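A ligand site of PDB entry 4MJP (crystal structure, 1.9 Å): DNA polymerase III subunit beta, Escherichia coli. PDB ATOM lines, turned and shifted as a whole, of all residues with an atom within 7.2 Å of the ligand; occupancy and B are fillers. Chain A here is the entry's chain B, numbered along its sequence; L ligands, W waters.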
ATOM      1  N   ARG A 152       0.221  17.799  -5.192  1.00  0.00           N
ATOM      2  CA  ARG A 152       0.989  16.641  -4.731  1.00  0.00           C
ATOM      3  C   ARG A 152       0.566  16.375  -3.291  1.00  0.00           C
ATOM      4  O   ARG A 152       1.186  16.824  -2.321  1.00  0.00           O
ATOM      5  CB  ARG A 152       2.478  16.899  -4.858  1.00  0.00           C
ATOM      6  CG  ARG A 152       2.930  17.084  -6.298  1.00  0.00           C
ATOM      7  CD  ARG A 152       4.340  17.638  -6.394  1.00  0.00           C
ATOM      8  NE  ARG A 152       4.451  18.957  -5.772  1.00  0.00           N
ATOM      9  CZ  ARG A 152       5.571  19.648  -5.661  1.00  0.00           C
ATOM     10  NH1 ARG A 152       6.719  19.169  -6.124  1.00  0.00           N
ATOM     11  NH2 ARG A 152       5.543  20.840  -5.077  1.00  0.00           N
ATOM     12  N   TYR A 154       0.512  13.991  -1.167  1.00  0.00           N
ATOM     13  CA  TYR A 154       1.417  13.318  -0.238  1.00  0.00           C
ATOM     14  C   TYR A 154       2.381  14.264   0.524  1.00  0.00           C
ATOM     15  O   TYR A 154       3.002  13.835   1.484  1.00  0.00           O
ATOM     16  CB  TYR A 154       2.243  12.226  -0.951  1.00  0.00           C
ATOM     17  CG  TYR A 154       2.940  12.723  -2.197  1.00  0.00           C
ATOM     18  CD1 TYR A 154       4.144  13.421  -2.106  1.00  0.00           C
ATOM     19  CD2 TYR A 154       2.388  12.525  -3.453  1.00  0.00           C
ATOM     20  CE1 TYR A 154       4.766  13.912  -3.242  1.00  0.00           C
ATOM     21  CE2 TYR A 154       2.993  12.999  -4.595  1.00  0.00           C
ATOM     22  CZ  TYR A 154       4.187  13.682  -4.479  1.00  0.00           C
ATOM     23  OH  TYR A 154       4.804  14.178  -5.594  1.00  0.00           O
ATOM     24  N   LEU A 155       2.474  15.520   0.094  1.00  0.00           N
ATOM     25  CA  LEU A 155       3.262  16.537   0.827  1.00  0.00           C
ATOM     26  C   LEU A 155       2.450  17.283   1.890  1.00  0.00           C
ATOM     27  O   LEU A 155       3.041  17.990   2.718  1.00  0.00           O
ATOM     28  CB  LEU A 155       3.848  17.555  -0.134  1.00  0.00           C
ATOM     29  CG  LEU A 155       4.722  17.034  -1.263  1.00  0.00           C
ATOM     30  CD1 LEU A 155       5.035  18.149  -2.244  1.00  0.00           C
ATOM     31  CD2 LEU A 155       5.984  16.422  -0.699  1.00  0.00           C
ATOM     32  N   VAL A 170       9.394  13.939   9.266  1.00  0.00           N
ATOM     33  CA  VAL A 170       9.933  14.627   8.120  1.00  0.00           C
ATOM     34  C   VAL A 170       8.822  15.426   7.463  1.00  0.00           C
ATOM     35  O   VAL A 170       7.703  14.932   7.343  1.00  0.00           O
ATOM     36  CB  VAL A 170      10.527  13.658   7.077  1.00  0.00           C
ATOM     37  CG1 VAL A 170      11.249  14.433   5.984  1.00  0.00           C
ATOM     38  CG2 VAL A 170      11.462  12.654   7.732  1.00  0.00           C
ATOM     39  N   ALA A 171       9.126  16.655   7.070  1.00  0.00           N
ATOM     40  CA  ALA A 171       8.177  17.490   6.373  1.00  0.00           C
ATOM     41  C   ALA A 171       8.861  18.284   5.276  1.00  0.00           C
ATOM     42  O   ALA A 171       9.996  18.770   5.435  1.00  0.00           O
ATOM     43  CB  ALA A 171       7.461  18.416   7.344  1.00  0.00           C
ATOM     44  N   THR A 172       8.184  18.377   4.144  1.00  0.00           N
ATOM     45  CA  THR A 172       8.624  19.226   3.067  1.00  0.00           C
ATOM     46  C   THR A 172       7.433  19.732   2.271  1.00  0.00           C
ATOM     47  O   THR A 172       6.380  19.079   2.182  1.00  0.00           O
ATOM     48  CB  THR A 172       9.630  18.504   2.144  1.00  0.00           C
ATOM     49  OG1 THR A 172      10.030  19.387   1.083  1.00  0.00           O
ATOM     50  CG2 THR A 172       9.022  17.252   1.537  1.00  0.00           C
ATOM     51  N   ASP A 173       7.610  20.927   1.715  1.00  0.00           N
ATOM     52  CA  ASP A 173       6.633  21.532   0.840  1.00  0.00           C
ATOM     53  C   ASP A 173       7.064  21.429  -0.608  1.00  0.00           C
ATOM     54  O   ASP A 173       6.493  22.102  -1.459  1.00  0.00           O
ATOM     55  CB  ASP A 173       6.397  22.988   1.229  1.00  0.00           C
ATOM     56  CG  ASP A 173       7.664  23.825   1.180  1.00  0.00           C
ATOM     57  OD1 ASP A 173       8.746  23.297   0.829  1.00  0.00           O
ATOM     58  OD2 ASP A 173       7.571  25.023   1.489  1.00  0.00           O
ATOM     59  N   GLY A 174       8.063  20.599  -0.891  1.00  0.00           N
ATOM     60  CA  GLY A 174       8.622  20.492  -2.224  1.00  0.00           C
ATOM     61  C   GLY A 174       9.788  21.440  -2.467  1.00  0.00           C
ATOM     62  O   GLY A 174      10.360  21.421  -3.543  1.00  0.00           O
ATOM     63  N   HIS A 175      10.158  22.260  -1.475  1.00  0.00           N
ATOM     64  CA  HIS A 175      11.219  23.253  -1.668  1.00  0.00           C
ATOM     65  C   HIS A 175      12.246  23.237  -0.541  1.00  0.00           C
ATOM     66  O   HIS A 175      13.440  23.234  -0.813  1.00  0.00           O
ATOM     67  CB  HIS A 175      10.623  24.653  -1.830  1.00  0.00           C
ATOM     68  CG  HIS A 175       9.653  24.727  -2.965  1.00  0.00           C
ATOM     69  ND1 HIS A 175      10.047  24.581  -4.277  1.00  0.00           N
ATOM     70  CD2 HIS A 175       8.316  24.845  -2.990  1.00  0.00           C
ATOM     71  CE1 HIS A 175       8.994  24.636  -5.062  1.00  0.00           C
ATOM     72  NE2 HIS A 175       7.921  24.796  -4.307  1.00  0.00           N
ATOM     73  N   ARG A 176      11.776  23.203   0.703  1.00  0.00           N
ATOM     74  CA  ARG A 176      12.651  23.107   1.872  1.00  0.00           C
ATOM     75  C   ARG A 176      12.238  21.929   2.758  1.00  0.00           C
ATOM     76  O   ARG A 176      11.118  21.417   2.660  1.00  0.00           O
ATOM     77  CB  ARG A 176      12.678  24.413   2.679  1.00  0.00           C
ATOM     78  CG  ARG A 176      11.380  25.211   2.724  1.00  0.00           C
ATOM     79  CD  ARG A 176      10.377  24.671   3.725  1.00  0.00           C
ATOM     80  NE  ARG A 176       9.162  25.493   3.729  1.00  0.00           N
ATOM     81  CZ  ARG A 176       8.999  26.621   4.421  1.00  0.00           C
ATOM     82  NH1 ARG A 176       9.966  27.088   5.196  1.00  0.00           N
ATOM     83  NH2 ARG A 176       7.848  27.288   4.331  1.00  0.00           N
ATOM     84  N   LEU A 177      13.158  21.488   3.589  1.00  0.00           N
ATOM     85  CA  LEU A 177      13.027  20.209   4.287  1.00  0.00           C
ATOM     86  C   LEU A 177      13.286  20.402   5.775  1.00  0.00           C
ATOM     87  O   LEU A 177      14.203  21.131   6.135  1.00  0.00           O
ATOM     88  CB  LEU A 177      14.056  19.209   3.766  1.00  0.00           C
ATOM     89  CG  LEU A 177      14.182  17.841   4.444  1.00  0.00           C
ATOM     90  CD1 LEU A 177      12.943  17.022   4.187  1.00  0.00           C
ATOM     91  CD2 LEU A 177      15.427  17.093   3.953  1.00  0.00           C
ATOM     92  N   ALA A 178      12.482  19.753   6.597  1.00  0.00           N
ATOM     93  CA  ALA A 178      12.706  19.668   8.048  1.00  0.00           C
ATOM     94  C   ALA A 178      12.675  18.195   8.463  1.00  0.00           C
ATOM     95  O   ALA A 178      11.802  17.453   8.022  1.00  0.00           O
ATOM     96  CB  ALA A 178      11.621  20.433   8.779  1.00  0.00           C
ATOM     97  N   ARG A 240       2.979   7.993  -1.540  1.00  0.00           N
ATOM     98  CA  ARG A 240       4.403   7.746  -1.326  1.00  0.00           C
ATOM     99  C   ARG A 240       5.065   9.071  -0.975  1.00  0.00           C
ATOM    100  O   ARG A 240       4.908  10.041  -1.711  1.00  0.00           O
ATOM    101  CB  ARG A 240       5.025   7.192  -2.610  1.00  0.00           C
ATOM    102  CG  ARG A 240       6.539   7.125  -2.568  1.00  0.00           C
ATOM    103  CD  ARG A 240       7.124   6.797  -3.937  1.00  0.00           C
ATOM    104  NE  ARG A 240       8.577   6.948  -3.933  1.00  0.00           N
ATOM    105  CZ  ARG A 240       9.226   8.104  -4.088  1.00  0.00           C
ATOM    106  NH1 ARG A 240       8.567   9.249  -4.253  1.00  0.00           N
ATOM    107  NH2 ARG A 240      10.556   8.112  -4.073  1.00  0.00           N
ATOM    108  N   PHE A 241       5.826   9.116   0.114  1.00  0.00           N
ATOM    109  CA  PHE A 241       6.569  10.325   0.458  1.00  0.00           C
ATOM    110  C   PHE A 241       7.824  10.434  -0.415  1.00  0.00           C
ATOM    111  O   PHE A 241       8.434   9.426  -0.737  1.00  0.00           O
ATOM    112  CB  PHE A 241       6.973  10.301   1.924  1.00  0.00           C
ATOM    113  CG  PHE A 241       7.248  11.666   2.504  1.00  0.00           C
ATOM    114  CD1 PHE A 241       6.195  12.513   2.807  1.00  0.00           C
ATOM    115  CD2 PHE A 241       8.531  12.078   2.769  1.00  0.00           C
ATOM    116  CE1 PHE A 241       6.433  13.769   3.365  1.00  0.00           C
ATOM    117  CE2 PHE A 241       8.777  13.330   3.315  1.00  0.00           C
ATOM    118  CZ  PHE A 241       7.731  14.165   3.618  1.00  0.00           C
ATOM    119  N   PRO A 242       8.232  11.672  -0.781  1.00  0.00           N
ATOM    120  CA  PRO A 242       9.447  11.790  -1.595  1.00  0.00           C
ATOM    121  C   PRO A 242      10.692  11.198  -0.936  1.00  0.00           C
ATOM    122  O   PRO A 242      10.785  11.111   0.287  1.00  0.00           O
ATOM    123  CB  PRO A 242       9.604  13.310  -1.765  1.00  0.00           C
ATOM    124  CG  PRO A 242       8.765  13.927  -0.705  1.00  0.00           C
ATOM    125  CD  PRO A 242       7.621  12.985  -0.519  1.00  0.00           C
ATOM    126  N   ASP A 243      11.640  10.756  -1.759  1.00  0.00           N
ATOM    127  CA  ASP A 243      12.896  10.233  -1.244  1.00  0.00           C
ATOM    128  C   ASP A 243      13.768  11.414  -0.803  1.00  0.00           C
ATOM    129  O   ASP A 243      14.735  11.784  -1.471  1.00  0.00           O
ATOM    130  CB  ASP A 243      13.593   9.380  -2.311  1.00  0.00           C
ATOM    131  CG  ASP A 243      14.827   8.673  -1.804  1.00  0.00           C
ATOM    132  OD1 ASP A 243      15.038   8.580  -0.566  1.00  0.00           O
ATOM    133  OD2 ASP A 243      15.600   8.190  -2.645  1.00  0.00           O
ATOM    134  N   TYR A 244      13.405  11.965   0.350  1.00  0.00           N
ATOM    135  CA  TYR A 244      14.020  13.175   0.898  1.00  0.00           C
ATOM    136  C   TYR A 244      15.533  13.009   1.176  1.00  0.00           C
ATOM    137  O   TYR A 244      16.287  13.969   1.139  1.00  0.00           O
ATOM    138  CB  TYR A 244      13.280  13.613   2.179  1.00  0.00           C
ATOM    139  CG  TYR A 244      13.536  12.708   3.370  1.00  0.00           C
ATOM    140  CD1 TYR A 244      14.590  12.968   4.238  1.00  0.00           C
ATOM    141  CD2 TYR A 244      12.736  11.584   3.629  1.00  0.00           C
ATOM    142  CE1 TYR A 244      14.853  12.160   5.326  1.00  0.00           C
ATOM    143  CE2 TYR A 244      12.990  10.756   4.700  1.00  0.00           C
ATOM    144  CZ  TYR A 244      14.042  11.056   5.554  1.00  0.00           C
ATOM    145  OH  TYR A 244      14.315  10.254   6.630  1.00  0.00           O
ATOM    146  N   ARG A 245      15.980  11.780   1.459  1.00  0.00           N
ATOM    147  CA  ARG A 245      17.407  11.532   1.744  1.00  0.00           C
ATOM    148  C   ARG A 245      18.346  12.000   0.641  1.00  0.00           C
ATOM    149  O   ARG A 245      19.491  12.373   0.900  1.00  0.00           O
ATOM    150  CB  ARG A 245      17.658  10.053   2.044  1.00  0.00           C
ATOM    151  CG  ARG A 245      17.125   9.614   3.392  1.00  0.00           C
ATOM    152  CD  ARG A 245      17.258   8.121   3.545  1.00  0.00           C
ATOM    153  NE  ARG A 245      16.907   7.655   4.885  1.00  0.00           N
ATOM    154  CZ  ARG A 245      15.661   7.444   5.312  1.00  0.00           C
ATOM    155  NH1 ARG A 245      14.619   7.675   4.539  1.00  0.00           N
ATOM    156  NH2 ARG A 245      15.467   7.006   6.552  1.00  0.00           N
ATOM    157  N   ARG A 246      17.847  12.011  -0.596  1.00  0.00           N
ATOM    158  CA  ARG A 246      18.624  12.460  -1.743  1.00  0.00           C
ATOM    159  C   ARG A 246      19.077  13.920  -1.676  1.00  0.00           C
ATOM    160  O   ARG A 246      20.088  14.265  -2.300  1.00  0.00           O
ATOM    161  CB  ARG A 246      17.841  12.222  -3.035  1.00  0.00           C
ATOM    162  CG  ARG A 246      17.661  10.747  -3.359  1.00  0.00           C
ATOM    163  CD  ARG A 246      16.514  10.486  -4.319  1.00  0.00           C
ATOM    164  NE  ARG A 246      16.659  11.182  -5.592  1.00  0.00           N
ATOM    165  CZ  ARG A 246      16.033  10.824  -6.724  1.00  0.00           C
ATOM    166  NH1 ARG A 246      16.236  11.532  -7.826  1.00  0.00           N
ATOM    167  NH2 ARG A 246      15.226   9.764  -6.748  1.00  0.00           N
ATOM    168  N   VAL A 247      18.369  14.778  -0.937  1.00  0.00           N
ATOM    169  CA  VAL A 247      18.794  16.180  -0.817  1.00  0.00           C
ATOM    170  C   VAL A 247      19.602  16.490   0.442  1.00  0.00           C
ATOM    171  O   VAL A 247      20.143  17.568   0.546  1.00  0.00           O
ATOM    172  CB  VAL A 247      17.603  17.166  -0.928  1.00  0.00           C
ATOM    173  CG1 VAL A 247      16.730  16.800  -2.115  1.00  0.00           C
ATOM    174  CG2 VAL A 247      16.803  17.236   0.371  1.00  0.00           C
ATOM    175  N   LEU A 248      19.687  15.561   1.397  1.00  0.00           N
ATOM    176  CA  LEU A 248      20.597  15.754   2.541  1.00  0.00           C
ATOM    177  C   LEU A 248      22.031  15.735   2.010  1.00  0.00           C
ATOM    178  O   LEU A 248      22.455  14.726   1.442  1.00  0.00           O
ATOM    179  CB  LEU A 248      20.434  14.641   3.580  1.00  0.00           C
ATOM    180  CG  LEU A 248      19.118  14.606   4.357  1.00  0.00           C
ATOM    181  CD1 LEU A 248      18.983  13.252   5.032  1.00  0.00           C
ATOM    182  CD2 LEU A 248      19.049  15.719   5.380  1.00  0.00           C
ATOM    183  N   VAL A 360      17.165  21.534   5.596  1.00  0.00           N
ATOM    184  CA  VAL A 360      17.870  21.702   4.328  1.00  0.00           C
ATOM    185  C   VAL A 360      17.167  22.749   3.451  1.00  0.00           C
ATOM    186  O   VAL A 360      15.942  22.694   3.231  1.00  0.00           O
ATOM    187  CB  VAL A 360      18.007  20.382   3.567  1.00  0.00           C
ATOM    188  CG1 VAL A 360      18.701  20.604   2.224  1.00  0.00           C
ATOM    189  CG2 VAL A 360      18.762  19.358   4.409  1.00  0.00           C
ATOM    190  N   MET A 362      17.662  24.880  -0.336  1.00  0.00           N
ATOM    191  CA  MET A 362      18.302  24.785  -1.657  1.00  0.00           C
ATOM    192  C   MET A 362      19.129  26.016  -1.984  1.00  0.00           C
ATOM    193  O   MET A 362      18.864  27.101  -1.471  1.00  0.00           O
ATOM    194  CB  MET A 362      17.231  24.661  -2.751  1.00  0.00           C
ATOM    195  CG  MET A 362      16.323  23.448  -2.645  1.00  0.00           C
ATOM    196  SD  MET A 362      17.244  21.958  -3.001  1.00  0.00           S
ATOM    197  CE  MET A 362      17.551  21.384  -1.338  1.00  0.00           C
HETATM  198  C1  LIG L   1      12.849  14.012  -3.962  1.00  0.00           C
HETATM  199  C2  LIG L   1      12.934  15.062  -3.031  1.00  0.00           C
HETATM  200  C3  LIG L   1      11.953  16.054  -2.891  1.00  0.00           C
HETATM  201  C4  LIG L   1      12.064  17.189  -1.902  1.00  0.00           C
HETATM  202  C5  LIG L   1      12.478  18.460  -2.653  1.00  0.00           C
HETATM  203  C6  LIG L   1      13.159  19.467  -0.329  1.00  0.00           C
HETATM  204  C7  LIG L   1      10.767  15.996  -3.810  1.00  0.00           C
HETATM  205  C8  LIG L   1       8.652  16.848  -4.635  1.00  0.00           C
HETATM  206  C9  LIG L   1       9.559  14.844  -5.650  1.00  0.00           C
HETATM  207  O1  LIG L   1       9.719  11.405  -5.967  1.00  0.00           O
HETATM  208  C10 LIG L   1      10.785  11.626  -5.407  1.00  0.00           C
HETATM  209  O2  LIG L   1      11.134  10.813  -4.410  1.00  0.00           O
HETATM  210  C11 LIG L   1      11.695  12.754  -5.856  1.00  0.00           C
HETATM  211  C12 LIG L   1      13.075  12.183  -6.189  1.00  0.00           C
HETATM  212  C13 LIG L   1      11.770  13.869  -4.856  1.00  0.00           C
HETATM  213  C14 LIG L   1      10.676  14.896  -4.807  1.00  0.00           C
HETATM  214  C15 LIG L   1       8.551  15.813  -5.564  1.00  0.00           C
HETATM  215  C16 LIG L   1       9.743  16.942  -3.770  1.00  0.00           C
HETATM  216  C17 LIG L   1      13.075  16.945  -0.791  1.00  0.00           C
HETATM  217  C18 LIG L   1      13.029  18.055   0.247  1.00  0.00           C
HETATM  218  C19 LIG L   1      13.157  19.568  -1.852  1.00  0.00           C
HETATM  219  O   HOH W   1       7.292  17.496  -8.321  1.00  0.00           O
HETATM  220  O   HOH W   2       7.640  12.444  -4.561  1.00  0.00           O
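Water W2 lies within hydrogen-bond range of an oxygen (O1) of the ligand (2.7 Å), the guanidinium group (NH1) of Arg 240 (3.3 Å) and the side-chain hydroxyl (OH) of Tyr 154 (3.5 Å).
NH1 of Arg 152 touches C8 of the ligand, at 3.4 Å.
Thr 172 touches the ligand.
Gly 174 touches the ligand (O to C5, 3.7 Å).
His 175 touches the ligand (O to C6, 3.8 Å).
CB of Leu 177 touches C18 of the ligand (3.8 Å).
CA of Pro 242 touches O2 of the ligand (3.4 Å).
NH2 of Arg 246 touches C12 of the ligand, 3.3 Å away.
Val 247 touches the ligand.
Ten residues have an atom within 4 Å of the ligand: Arg 152, Thr 172, Gly 174, His 175, Leu 177, Arg 240, Pro 242, Asp 243, Arg 246 and Val 247.
N of Gly 174 sits at hydrogen-bond distance from OG1 of Thr 172, 3.0 Å away.
The side-chain hydroxyl (OG1) of Thr 172 sits at hydrogen-bond distance from the backbone carbonyl oxygen (O) of Arg 176 (2.8 Å).
The backbone NH (N) of His 175 lies within hydrogen-bond range of the side-chain carboxylate (OD1) of Asp 173 (2.9 Å).
The backbone NH (N) of Val 360 sits at hydrogen-bond distance from the backbone carbonyl oxygen (O) of Leu 177 (3.0 Å).
An oxygen (O2) of the ligand lies within hydrogen-bond range of the backbone NH (N) of Asp 243 (2.7 Å).
O2 of the ligand is in salt-bridge range of NH2 of Arg 240 (2.8 Å).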
